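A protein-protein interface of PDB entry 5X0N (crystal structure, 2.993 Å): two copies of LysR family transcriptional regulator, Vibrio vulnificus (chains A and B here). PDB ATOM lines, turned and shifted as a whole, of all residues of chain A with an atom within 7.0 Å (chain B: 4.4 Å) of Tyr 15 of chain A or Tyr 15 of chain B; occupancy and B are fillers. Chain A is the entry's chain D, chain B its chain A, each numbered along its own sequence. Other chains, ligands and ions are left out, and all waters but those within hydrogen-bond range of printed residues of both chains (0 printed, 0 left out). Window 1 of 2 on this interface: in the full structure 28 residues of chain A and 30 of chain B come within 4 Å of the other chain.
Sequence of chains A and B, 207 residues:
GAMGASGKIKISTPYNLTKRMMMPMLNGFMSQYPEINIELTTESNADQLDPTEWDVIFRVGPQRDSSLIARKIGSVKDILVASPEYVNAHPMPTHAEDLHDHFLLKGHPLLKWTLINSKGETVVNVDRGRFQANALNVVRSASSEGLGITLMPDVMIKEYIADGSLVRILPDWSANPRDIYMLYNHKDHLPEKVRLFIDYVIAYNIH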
ATOM      1  N   THR A  13     -17.709  15.928  -4.501  1.00  0.00           N
ATOM      2  CA  THR A  13     -17.898  14.672  -3.788  1.00  0.00           C
ATOM      3  C   THR A  13     -19.100  13.940  -4.366  1.00  0.00           C
ATOM      4  O   THR A  13     -20.088  14.590  -4.734  1.00  0.00           O
ATOM      5  CB  THR A  13     -18.105  14.915  -2.285  1.00  0.00           C
ATOM      6  OG1 THR A  13     -16.963  15.596  -1.749  1.00  0.00           O
ATOM      7  CG2 THR A  13     -18.291  13.610  -1.536  1.00  0.00           C
ATOM      8  N   PRO A  14     -19.039  12.611  -4.490  1.00  0.00           N
ATOM      9  CA  PRO A  14     -20.225  11.854  -4.904  1.00  0.00           C
ATOM     10  C   PRO A  14     -21.413  12.110  -3.986  1.00  0.00           C
ATOM     11  O   PRO A  14     -21.261  12.467  -2.815  1.00  0.00           O
ATOM     12  CB  PRO A  14     -19.759  10.396  -4.825  1.00  0.00           C
ATOM     13  CG  PRO A  14     -18.291  10.472  -5.072  1.00  0.00           C
ATOM     14  CD  PRO A  14     -17.830  11.765  -4.455  1.00  0.00           C
ATOM     15  N   TYR A  15     -22.610  11.907  -4.539  1.00  0.00           N
ATOM     16  CA  TYR A  15     -23.837  12.294  -3.849  1.00  0.00           C
ATOM     17  C   TYR A  15     -24.103  11.413  -2.633  1.00  0.00           C
ATOM     18  O   TYR A  15     -24.299  11.916  -1.521  1.00  0.00           O
ATOM     19  CB  TYR A  15     -25.014  12.231  -4.825  1.00  0.00           C
ATOM     20  CG  TYR A  15     -26.206  13.090  -4.453  1.00  0.00           C
ATOM     21  CD1 TYR A  15     -26.879  12.904  -3.252  1.00  0.00           C
ATOM     22  CD2 TYR A  15     -26.663  14.082  -5.312  1.00  0.00           C
ATOM     23  CE1 TYR A  15     -27.967  13.683  -2.915  1.00  0.00           C
ATOM     24  CE2 TYR A  15     -27.752  14.868  -4.982  1.00  0.00           C
ATOM     25  CZ  TYR A  15     -28.400  14.664  -3.782  1.00  0.00           C
ATOM     26  OH  TYR A  15     -29.484  15.441  -3.446  1.00  0.00           O
ATOM     27  N   ASN A  16     -24.115  10.094  -2.824  1.00  0.00           N
ATOM     28  CA  ASN A  16     -24.677   9.189  -1.827  1.00  0.00           C
ATOM     29  C   ASN A  16     -23.681   8.751  -0.761  1.00  0.00           C
ATOM     30  O   ASN A  16     -24.084   8.519   0.386  1.00  0.00           O
ATOM     31  CB  ASN A  16     -25.256   7.953  -2.520  1.00  0.00           C
ATOM     32  CG  ASN A  16     -26.272   8.309  -3.585  1.00  0.00           C
ATOM     33  OD1 ASN A  16     -27.404   8.685  -3.280  1.00  0.00           O
ATOM     34  ND2 ASN A  16     -25.872   8.199  -4.847  1.00  0.00           N
ATOM     35  N   LEU A  17     -22.401   8.632  -1.099  1.00  0.00           N
ATOM     36  CA  LEU A  17     -21.409   8.076  -0.190  1.00  0.00           C
ATOM     37  C   LEU A  17     -20.679   9.136   0.625  1.00  0.00           C
ATOM     38  O   LEU A  17     -19.651   8.830   1.238  1.00  0.00           O
ATOM     39  CB  LEU A  17     -20.400   7.239  -0.974  1.00  0.00           C
ATOM     40  CG  LEU A  17     -21.032   6.113  -1.788  1.00  0.00           C
ATOM     41  CD1 LEU A  17     -20.895   6.373  -3.278  1.00  0.00           C
ATOM     42  CD2 LEU A  17     -20.397   4.804  -1.413  1.00  0.00           C
ATOM     43  N   THR A  18     -21.189  10.367   0.653  1.00  0.00           N
ATOM     44  CA  THR A  18     -20.495  11.444   1.352  1.00  0.00           C
ATOM     45  C   THR A  18     -20.563  11.261   2.862  1.00  0.00           C
ATOM     46  O   THR A  18     -19.551  11.396   3.563  1.00  0.00           O
ATOM     47  CB  THR A  18     -21.096  12.795   0.961  1.00  0.00           C
ATOM     48  OG1 THR A  18     -21.191  12.886  -0.465  1.00  0.00           O
ATOM     49  CG2 THR A  18     -20.238  13.934   1.491  1.00  0.00           C
ATOM     50  N   LYS A  19     -21.751  10.950   3.381  1.00  0.00           N
ATOM     51  CA  LYS A  19     -21.984  11.021   4.820  1.00  0.00           C
ATOM     52  C   LYS A  19     -21.180   9.981   5.594  1.00  0.00           C
ATOM     53  O   LYS A  19     -20.742  10.255   6.717  1.00  0.00           O
ATOM     54  CB  LYS A  19     -23.477  10.860   5.107  1.00  0.00           C
ATOM     55  CG  LYS A  19     -24.013  11.787   6.184  1.00  0.00           C
ATOM     56  CD  LYS A  19     -23.576  11.317   7.557  1.00  0.00           C
ATOM     57  CE  LYS A  19     -24.397  11.938   8.664  1.00  0.00           C
ATOM     58  NZ  LYS A  19     -24.191  11.180   9.928  1.00  0.00           N
ATOM     59  N   THR A  41     -19.296  20.148  -2.306  1.00  0.00           N
ATOM     60  CA  THR A  41     -20.408  20.077  -3.239  1.00  0.00           C
ATOM     61  C   THR A  41     -20.692  18.618  -3.559  1.00  0.00           C
ATOM     62  O   THR A  41     -19.769  17.840  -3.814  1.00  0.00           O
ATOM     63  CB  THR A  41     -20.106  20.850  -4.526  1.00  0.00           C
ATOM     64  OG1 THR A  41     -19.767  22.204  -4.202  1.00  0.00           O
ATOM     65  CG2 THR A  41     -21.315  20.846  -5.446  1.00  0.00           C
ATOM     66  N   THR A  42     -21.970  18.252  -3.533  1.00  0.00           N
ATOM     67  CA  THR A  42     -22.401  16.898  -3.852  1.00  0.00           C
ATOM     68  C   THR A  42     -22.962  16.868  -5.267  1.00  0.00           C
ATOM     69  O   THR A  42     -23.844  17.663  -5.611  1.00  0.00           O
ATOM     70  CB  THR A  42     -23.444  16.400  -2.850  1.00  0.00           C
ATOM     71  OG1 THR A  42     -24.361  17.457  -2.540  1.00  0.00           O
ATOM     72  CG2 THR A  42     -22.763  15.937  -1.570  1.00  0.00           C
ATOM     73  N   GLU A  43     -22.446  15.952  -6.081  1.00  0.00           N
ATOM     74  CA  GLU A  43     -22.743  15.888  -7.502  1.00  0.00           C
ATOM     75  C   GLU A  43     -23.287  14.511  -7.863  1.00  0.00           C
ATOM     76  O   GLU A  43     -23.030  13.517  -7.178  1.00  0.00           O
ATOM     77  CB  GLU A  43     -21.487  16.197  -8.334  1.00  0.00           C
ATOM     78  CG  GLU A  43     -21.723  16.361  -9.828  1.00  0.00           C
ATOM     79  CD  GLU A  43     -21.840  17.812 -10.246  1.00  0.00           C
ATOM     80  OE1 GLU A  43     -22.448  18.078 -11.304  1.00  0.00           O
ATOM     81  OE2 GLU A  43     -21.323  18.685  -9.517  1.00  0.00           O
ATOM     82  N   SER A  44     -24.055  14.468  -8.950  1.00  0.00           N
ATOM     83  CA  SER A  44     -24.560  13.221  -9.513  1.00  0.00           C
ATOM     84  C   SER A  44     -23.758  12.751 -10.719  1.00  0.00           C
ATOM     85  O   SER A  44     -23.450  11.561 -10.823  1.00  0.00           O
ATOM     86  CB  SER A  44     -26.031  13.377  -9.911  1.00  0.00           C
ATOM     87  OG  SER A  44     -26.863  13.444  -8.766  1.00  0.00           O
ATOM     88  N   HIS A 108     -30.261   6.391  -8.192  1.00  0.00           N
ATOM     89  CA  HIS A 108     -29.066   6.832  -8.897  1.00  0.00           C
ATOM     90  C   HIS A 108     -27.843   6.685  -7.994  1.00  0.00           C
ATOM     91  O   HIS A 108     -27.896   7.044  -6.814  1.00  0.00           O
ATOM     92  CB  HIS A 108     -29.223   8.285  -9.341  1.00  0.00           C
ATOM     93  CG  HIS A 108     -28.179   8.742 -10.310  1.00  0.00           C
ATOM     94  ND1 HIS A 108     -26.903   9.090  -9.921  1.00  0.00           N
ATOM     95  CD2 HIS A 108     -28.223   8.915 -11.653  1.00  0.00           C
ATOM     96  CE1 HIS A 108     -26.206   9.453 -10.983  1.00  0.00           C
ATOM     97  NE2 HIS A 108     -26.983   9.355 -12.046  1.00  0.00           N
ATOM     98  N   PRO A 109     -26.715   6.181  -8.520  1.00  0.00           N
ATOM     99  CA  PRO A 109     -26.499   5.802  -9.920  1.00  0.00           C
ATOM    100  C   PRO A 109     -26.691   4.314 -10.220  1.00  0.00           C
ATOM    101  O   PRO A 109     -26.000   3.782 -11.089  1.00  0.00           O
ATOM    102  CB  PRO A 109     -25.043   6.201 -10.143  1.00  0.00           C
ATOM    103  CG  PRO A 109     -24.399   5.909  -8.818  1.00  0.00           C
ATOM    104  CD  PRO A 109     -25.460   6.122  -7.750  1.00  0.00           C
ATOM    105  N   ASN A 134     -33.070   9.885  -7.674  1.00  0.00           N
ATOM    106  CA  ASN A 134     -31.722  10.345  -7.980  1.00  0.00           C
ATOM    107  C   ASN A 134     -30.789  10.289  -6.778  1.00  0.00           C
ATOM    108  O   ASN A 134     -29.602  10.604  -6.913  1.00  0.00           O
ATOM    109  CB  ASN A 134     -31.760  11.772  -8.544  1.00  0.00           C
ATOM    110  CG  ASN A 134     -32.217  12.796  -7.523  1.00  0.00           C
ATOM    111  OD1 ASN A 134     -32.814  12.454  -6.503  1.00  0.00           O
ATOM    112  ND2 ASN A 134     -31.943  14.066  -7.799  1.00  0.00           N
ATOM    113  N   ALA A 135     -31.295   9.906  -5.610  1.00  0.00           N
ATOM    114  CA  ALA A 135     -30.484   9.673  -4.428  1.00  0.00           C
ATOM    115  C   ALA A 135     -30.689   8.239  -3.959  1.00  0.00           C
ATOM    116  O   ALA A 135     -31.643   7.565  -4.354  1.00  0.00           O
ATOM    117  CB  ALA A 135     -30.831  10.657  -3.304  1.00  0.00           C
ATOM    118  N   LEU A 136     -29.775   7.771  -3.112  1.00  0.00           N
ATOM    119  CA  LEU A 136     -29.830   6.408  -2.597  1.00  0.00           C
ATOM    120  C   LEU A 136     -30.298   6.319  -1.157  1.00  0.00           C
ATOM    121  O   LEU A 136     -31.023   5.385  -0.810  1.00  0.00           O
ATOM    122  CB  LEU A 136     -28.459   5.736  -2.721  1.00  0.00           C
ATOM    123  CG  LEU A 136     -28.130   5.245  -4.129  1.00  0.00           C
ATOM    124  CD1 LEU A 136     -26.717   4.692  -4.188  1.00  0.00           C
ATOM    125  CD2 LEU A 136     -29.142   4.203  -4.578  1.00  0.00           C
ATOM    126  N   ASN A 137     -29.911   7.272  -0.305  1.00  0.00           N
ATOM    127  CA  ASN A 137     -30.396   7.282   1.070  1.00  0.00           C
ATOM    128  C   ASN A 137     -31.915   7.284   1.133  1.00  0.00           C
ATOM    129  O   ASN A 137     -32.489   6.934   2.171  1.00  0.00           O
ATOM    130  CB  ASN A 137     -29.843   8.506   1.814  1.00  0.00           C
ATOM    131  CG  ASN A 137     -30.273   9.824   1.187  1.00  0.00           C
ATOM    132  OD1 ASN A 137     -30.607   9.884   0.008  1.00  0.00           O
ATOM    133  ND2 ASN A 137     -30.276  10.889   1.989  1.00  0.00           N
ATOM    134  N   THR B  13     -38.515  17.598  -4.890  1.00  0.00           N
ATOM    135  CA  THR B  13     -38.491  17.955  -3.478  1.00  0.00           C
ATOM    136  C   THR B  13     -37.174  18.635  -3.142  1.00  0.00           C
ATOM    137  O   THR B  13     -36.167  18.414  -3.826  1.00  0.00           O
ATOM    138  CB  THR B  13     -38.660  16.721  -2.574  1.00  0.00           C
ATOM    139  OG1 THR B  13     -37.675  15.737  -2.915  1.00  0.00           O
ATOM    140  CG2 THR B  13     -40.052  16.121  -2.724  1.00  0.00           C
ATOM    141  N   PRO B  14     -37.148  19.471  -2.101  1.00  0.00           N
ATOM    142  CA  PRO B  14     -35.865  19.988  -1.612  1.00  0.00           C
ATOM    143  C   PRO B  14     -35.070  18.887  -0.925  1.00  0.00           C
ATOM    144  O   PRO B  14     -35.629  18.037  -0.228  1.00  0.00           O
ATOM    145  CB  PRO B  14     -36.275  21.091  -0.631  1.00  0.00           C
ATOM    146  CG  PRO B  14     -37.640  20.696  -0.177  1.00  0.00           C
ATOM    147  CD  PRO B  14     -38.291  20.035  -1.362  1.00  0.00           C
ATOM    148  N   TYR B  15     -33.750  18.914  -1.129  1.00  0.00           N
ATOM    149  CA  TYR B  15     -32.899  17.811  -0.689  1.00  0.00           C
ATOM    150  C   TYR B  15     -32.955  17.627   0.823  1.00  0.00           C
ATOM    151  O   TYR B  15     -33.247  16.534   1.318  1.00  0.00           O
ATOM    152  CB  TYR B  15     -31.459  18.053  -1.158  1.00  0.00           C
ATOM    153  CG  TYR B  15     -30.439  17.008  -0.738  1.00  0.00           C
ATOM    154  CD1 TYR B  15     -30.821  15.712  -0.410  1.00  0.00           C
ATOM    155  CD2 TYR B  15     -29.088  17.321  -0.685  1.00  0.00           C
ATOM    156  CE1 TYR B  15     -29.887  14.765  -0.025  1.00  0.00           C
ATOM    157  CE2 TYR B  15     -28.148  16.381  -0.309  1.00  0.00           C
ATOM    158  CZ  TYR B  15     -28.552  15.106   0.022  1.00  0.00           C
ATOM    159  OH  TYR B  15     -27.613  14.172   0.398  1.00  0.00           O
ATOM    160  N   ASN B  16     -32.685  18.689   1.574  1.00  0.00           N
ATOM    161  CA  ASN B  16     -32.437  18.552   3.007  1.00  0.00           C
ATOM    162  C   ASN B  16     -33.681  18.099   3.761  1.00  0.00           C
ATOM    163  O   ASN B  16     -33.604  17.221   4.626  1.00  0.00           O
ATOM    164  CB  ASN B  16     -31.909  19.875   3.568  1.00  0.00           C
ATOM    165  CG  ASN B  16     -30.520  20.201   3.062  1.00  0.00           C
ATOM    166  OD1 ASN B  16     -29.577  19.447   3.271  1.00  0.00           O
ATOM    167  ND2 ASN B  16     -30.388  21.346   2.393  1.00  0.00           N
ATOM    168  N   LEU B  17     -34.835  18.673   3.441  1.00  0.00           N
ATOM    169  CA  LEU B  17     -36.063  18.328   4.145  1.00  0.00           C
ATOM    170  C   LEU B  17     -36.693  17.024   3.667  1.00  0.00           C
ATOM    171  O   LEU B  17     -37.751  16.642   4.184  1.00  0.00           O
ATOM    172  CB  LEU B  17     -37.082  19.462   4.015  1.00  0.00           C
ATOM    173  CG  LEU B  17     -36.630  20.824   4.543  1.00  0.00           C
ATOM    174  CD1 LEU B  17     -37.284  21.938   3.749  1.00  0.00           C
ATOM    175  CD2 LEU B  17     -36.944  20.955   6.025  1.00  0.00           C
ATOM    176  N   THR B  18     -36.078  16.330   2.708  1.00  0.00           N
ATOM    177  CA  THR B  18     -36.708  15.143   2.136  1.00  0.00           C
ATOM    178  C   THR B  18     -36.699  13.971   3.114  1.00  0.00           C
ATOM    179  O   THR B  18     -37.671  13.209   3.185  1.00  0.00           O
ATOM    180  CB  THR B  18     -36.009  14.760   0.827  1.00  0.00           C
ATOM    181  OG1 THR B  18     -36.318  15.731  -0.180  1.00  0.00           O
ATOM    182  CG2 THR B  18     -36.459  13.387   0.347  1.00  0.00           C
ATOM    183  N   THR B  42     -34.348  15.060  -5.888  1.00  0.00           N
ATOM    184  CA  THR B  42     -34.134  16.047  -4.837  1.00  0.00           C
ATOM    185  C   THR B  42     -33.220  17.146  -5.357  1.00  0.00           C
ATOM    186  O   THR B  42     -32.179  16.861  -5.958  1.00  0.00           O
ATOM    187  CB  THR B  42     -33.529  15.393  -3.595  1.00  0.00           C
ATOM    188  OG1 THR B  42     -32.170  15.024  -3.862  1.00  0.00           O
ATOM    189  CG2 THR B  42     -34.317  14.150  -3.214  1.00  0.00           C
ATOM    190  N   GLU B  43     -33.608  18.397  -5.125  1.00  0.00           N
ATOM    191  CA  GLU B  43     -32.867  19.532  -5.665  1.00  0.00           C
ATOM    192  C   GLU B  43     -32.012  20.218  -4.605  1.00  0.00           C
ATOM    193  O   GLU B  43     -32.278  20.103  -3.410  1.00  0.00           O
ATOM    194  CB  GLU B  43     -33.831  20.543  -6.291  1.00  0.00           C
ATOM    195  CG  GLU B  43     -35.064  19.916  -6.929  1.00  0.00           C
ATOM    196  CD  GLU B  43     -34.801  19.351  -8.315  1.00  0.00           C
ATOM    197  OE1 GLU B  43     -35.779  19.126  -9.059  1.00  0.00           O
ATOM    198  OE2 GLU B  43     -33.621  19.131  -8.664  1.00  0.00           O
ATOM    199  N   ALA B 135     -25.483  20.777   1.126  1.00  0.00           N
ATOM    200  CA  ALA B 135     -26.429  19.989   1.901  1.00  0.00           C
ATOM    201  C   ALA B 135     -26.259  20.295   3.383  1.00  0.00           C
ATOM    202  O   ALA B 135     -25.264  20.886   3.811  1.00  0.00           O
ATOM    203  CB  ALA B 135     -26.238  18.488   1.643  1.00  0.00           C
ATOM    204  N   ASN B 137     -27.334  17.679   5.945  1.00  0.00           N
ATOM    205  CA  ASN B 137     -27.009  16.451   6.664  1.00  0.00           C
ATOM    206  C   ASN B 137     -25.506  16.307   6.861  1.00  0.00           C
ATOM    207  O   ASN B 137     -25.056  15.804   7.897  1.00  0.00           O
ATOM    208  CB  ASN B 137     -27.565  15.235   5.919  1.00  0.00           C
ATOM    209  CG  ASN B 137     -26.812  14.943   4.630  1.00  0.00           C
ATOM    210  OD1 ASN B 137     -26.514  15.853   3.854  1.00  0.00           O
ATOM    211  ND2 ASN B 137     -26.497  13.673   4.401  1.00  0.00           N
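Among the printed residues, merely in contact across the chains: Tyr 15 of chain A with Tyr 15 of chain B (3.3 Å) and Lys 19 of chain A with Asn 137 of chain B (3.6 Å).
The side-chain hydroxyl of Thr 18 of chain A sits at hydrogen-bond distance from the backbone carbonyl oxygen of Tyr 15 of chain A (3.4 Å).
The backbone NH (N) of Tyr 15 of chain B sits at hydrogen-bond distance from the backbone carbonyl oxygen (O) of Glu 43 of chain B (3.0 Å).
The backbone carbonyl oxygen (O) of Glu 43 of chain A is in hydrogen-bond range of the backbone NH (N) of Tyr 15 of chain A (3.1 Å).
Tyr 15 of chain B touches its own counterpart, Tyr 15 of chain A.
Tyr 15 of chain A touches Thr 42 of chain B, but with the chains exchanged Thr 42 of chain A does not touch Tyr 15 of chain B (4.5 Å).
Of the 4 pairs that touch across the chains among the printed residues, 1 has its exchanged pair printed and touching as well.
Of chain B, only Tyr 15 and Thr 42 come within 4 Å of Tyr 15 of chain A.
Printed residues of chain B within 4 Å of Lys 19 of chain A: Asn 137 (3.6 Å).
Of the printed residues of chain B, Asn 134 of chain A touches Thr 42.
Tyr 15 of chain B touches just one residue of chain A: Tyr 15.
Of the printed residues of chain A, Thr 42 of chain B touches Tyr 15 and Asn 134.
Of the printed residues of chain A, Asn 137 of chain B touches Lys 19 (3.6 Å).
N of Thr 42 of chain B lies within hydrogen-bond range of OD1 of Asn 134 of chain A (3.1 Å).
The side-chain hydroxyl (OG1) of Thr 42 of chain B sits at hydrogen-bond distance from the side-chain hydroxyl (OH) of Tyr 15 of chain A.
Of the 17 printed residues of chain A, 3 touch a printed residue of chain B.
Hydrophobic or aromatic side chains of chain A that line the printed part of chain B: Tyr 15.
Printed residues of chain B that touch a printed residue of chain A: Tyr 15, Thr 42 and Asn 137.
Hydrophobic or aromatic side chains of chain B within 4 Å of the printed part of chain A: Tyr 15.
Among the printed residues, 4 pairs touch across the chains.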
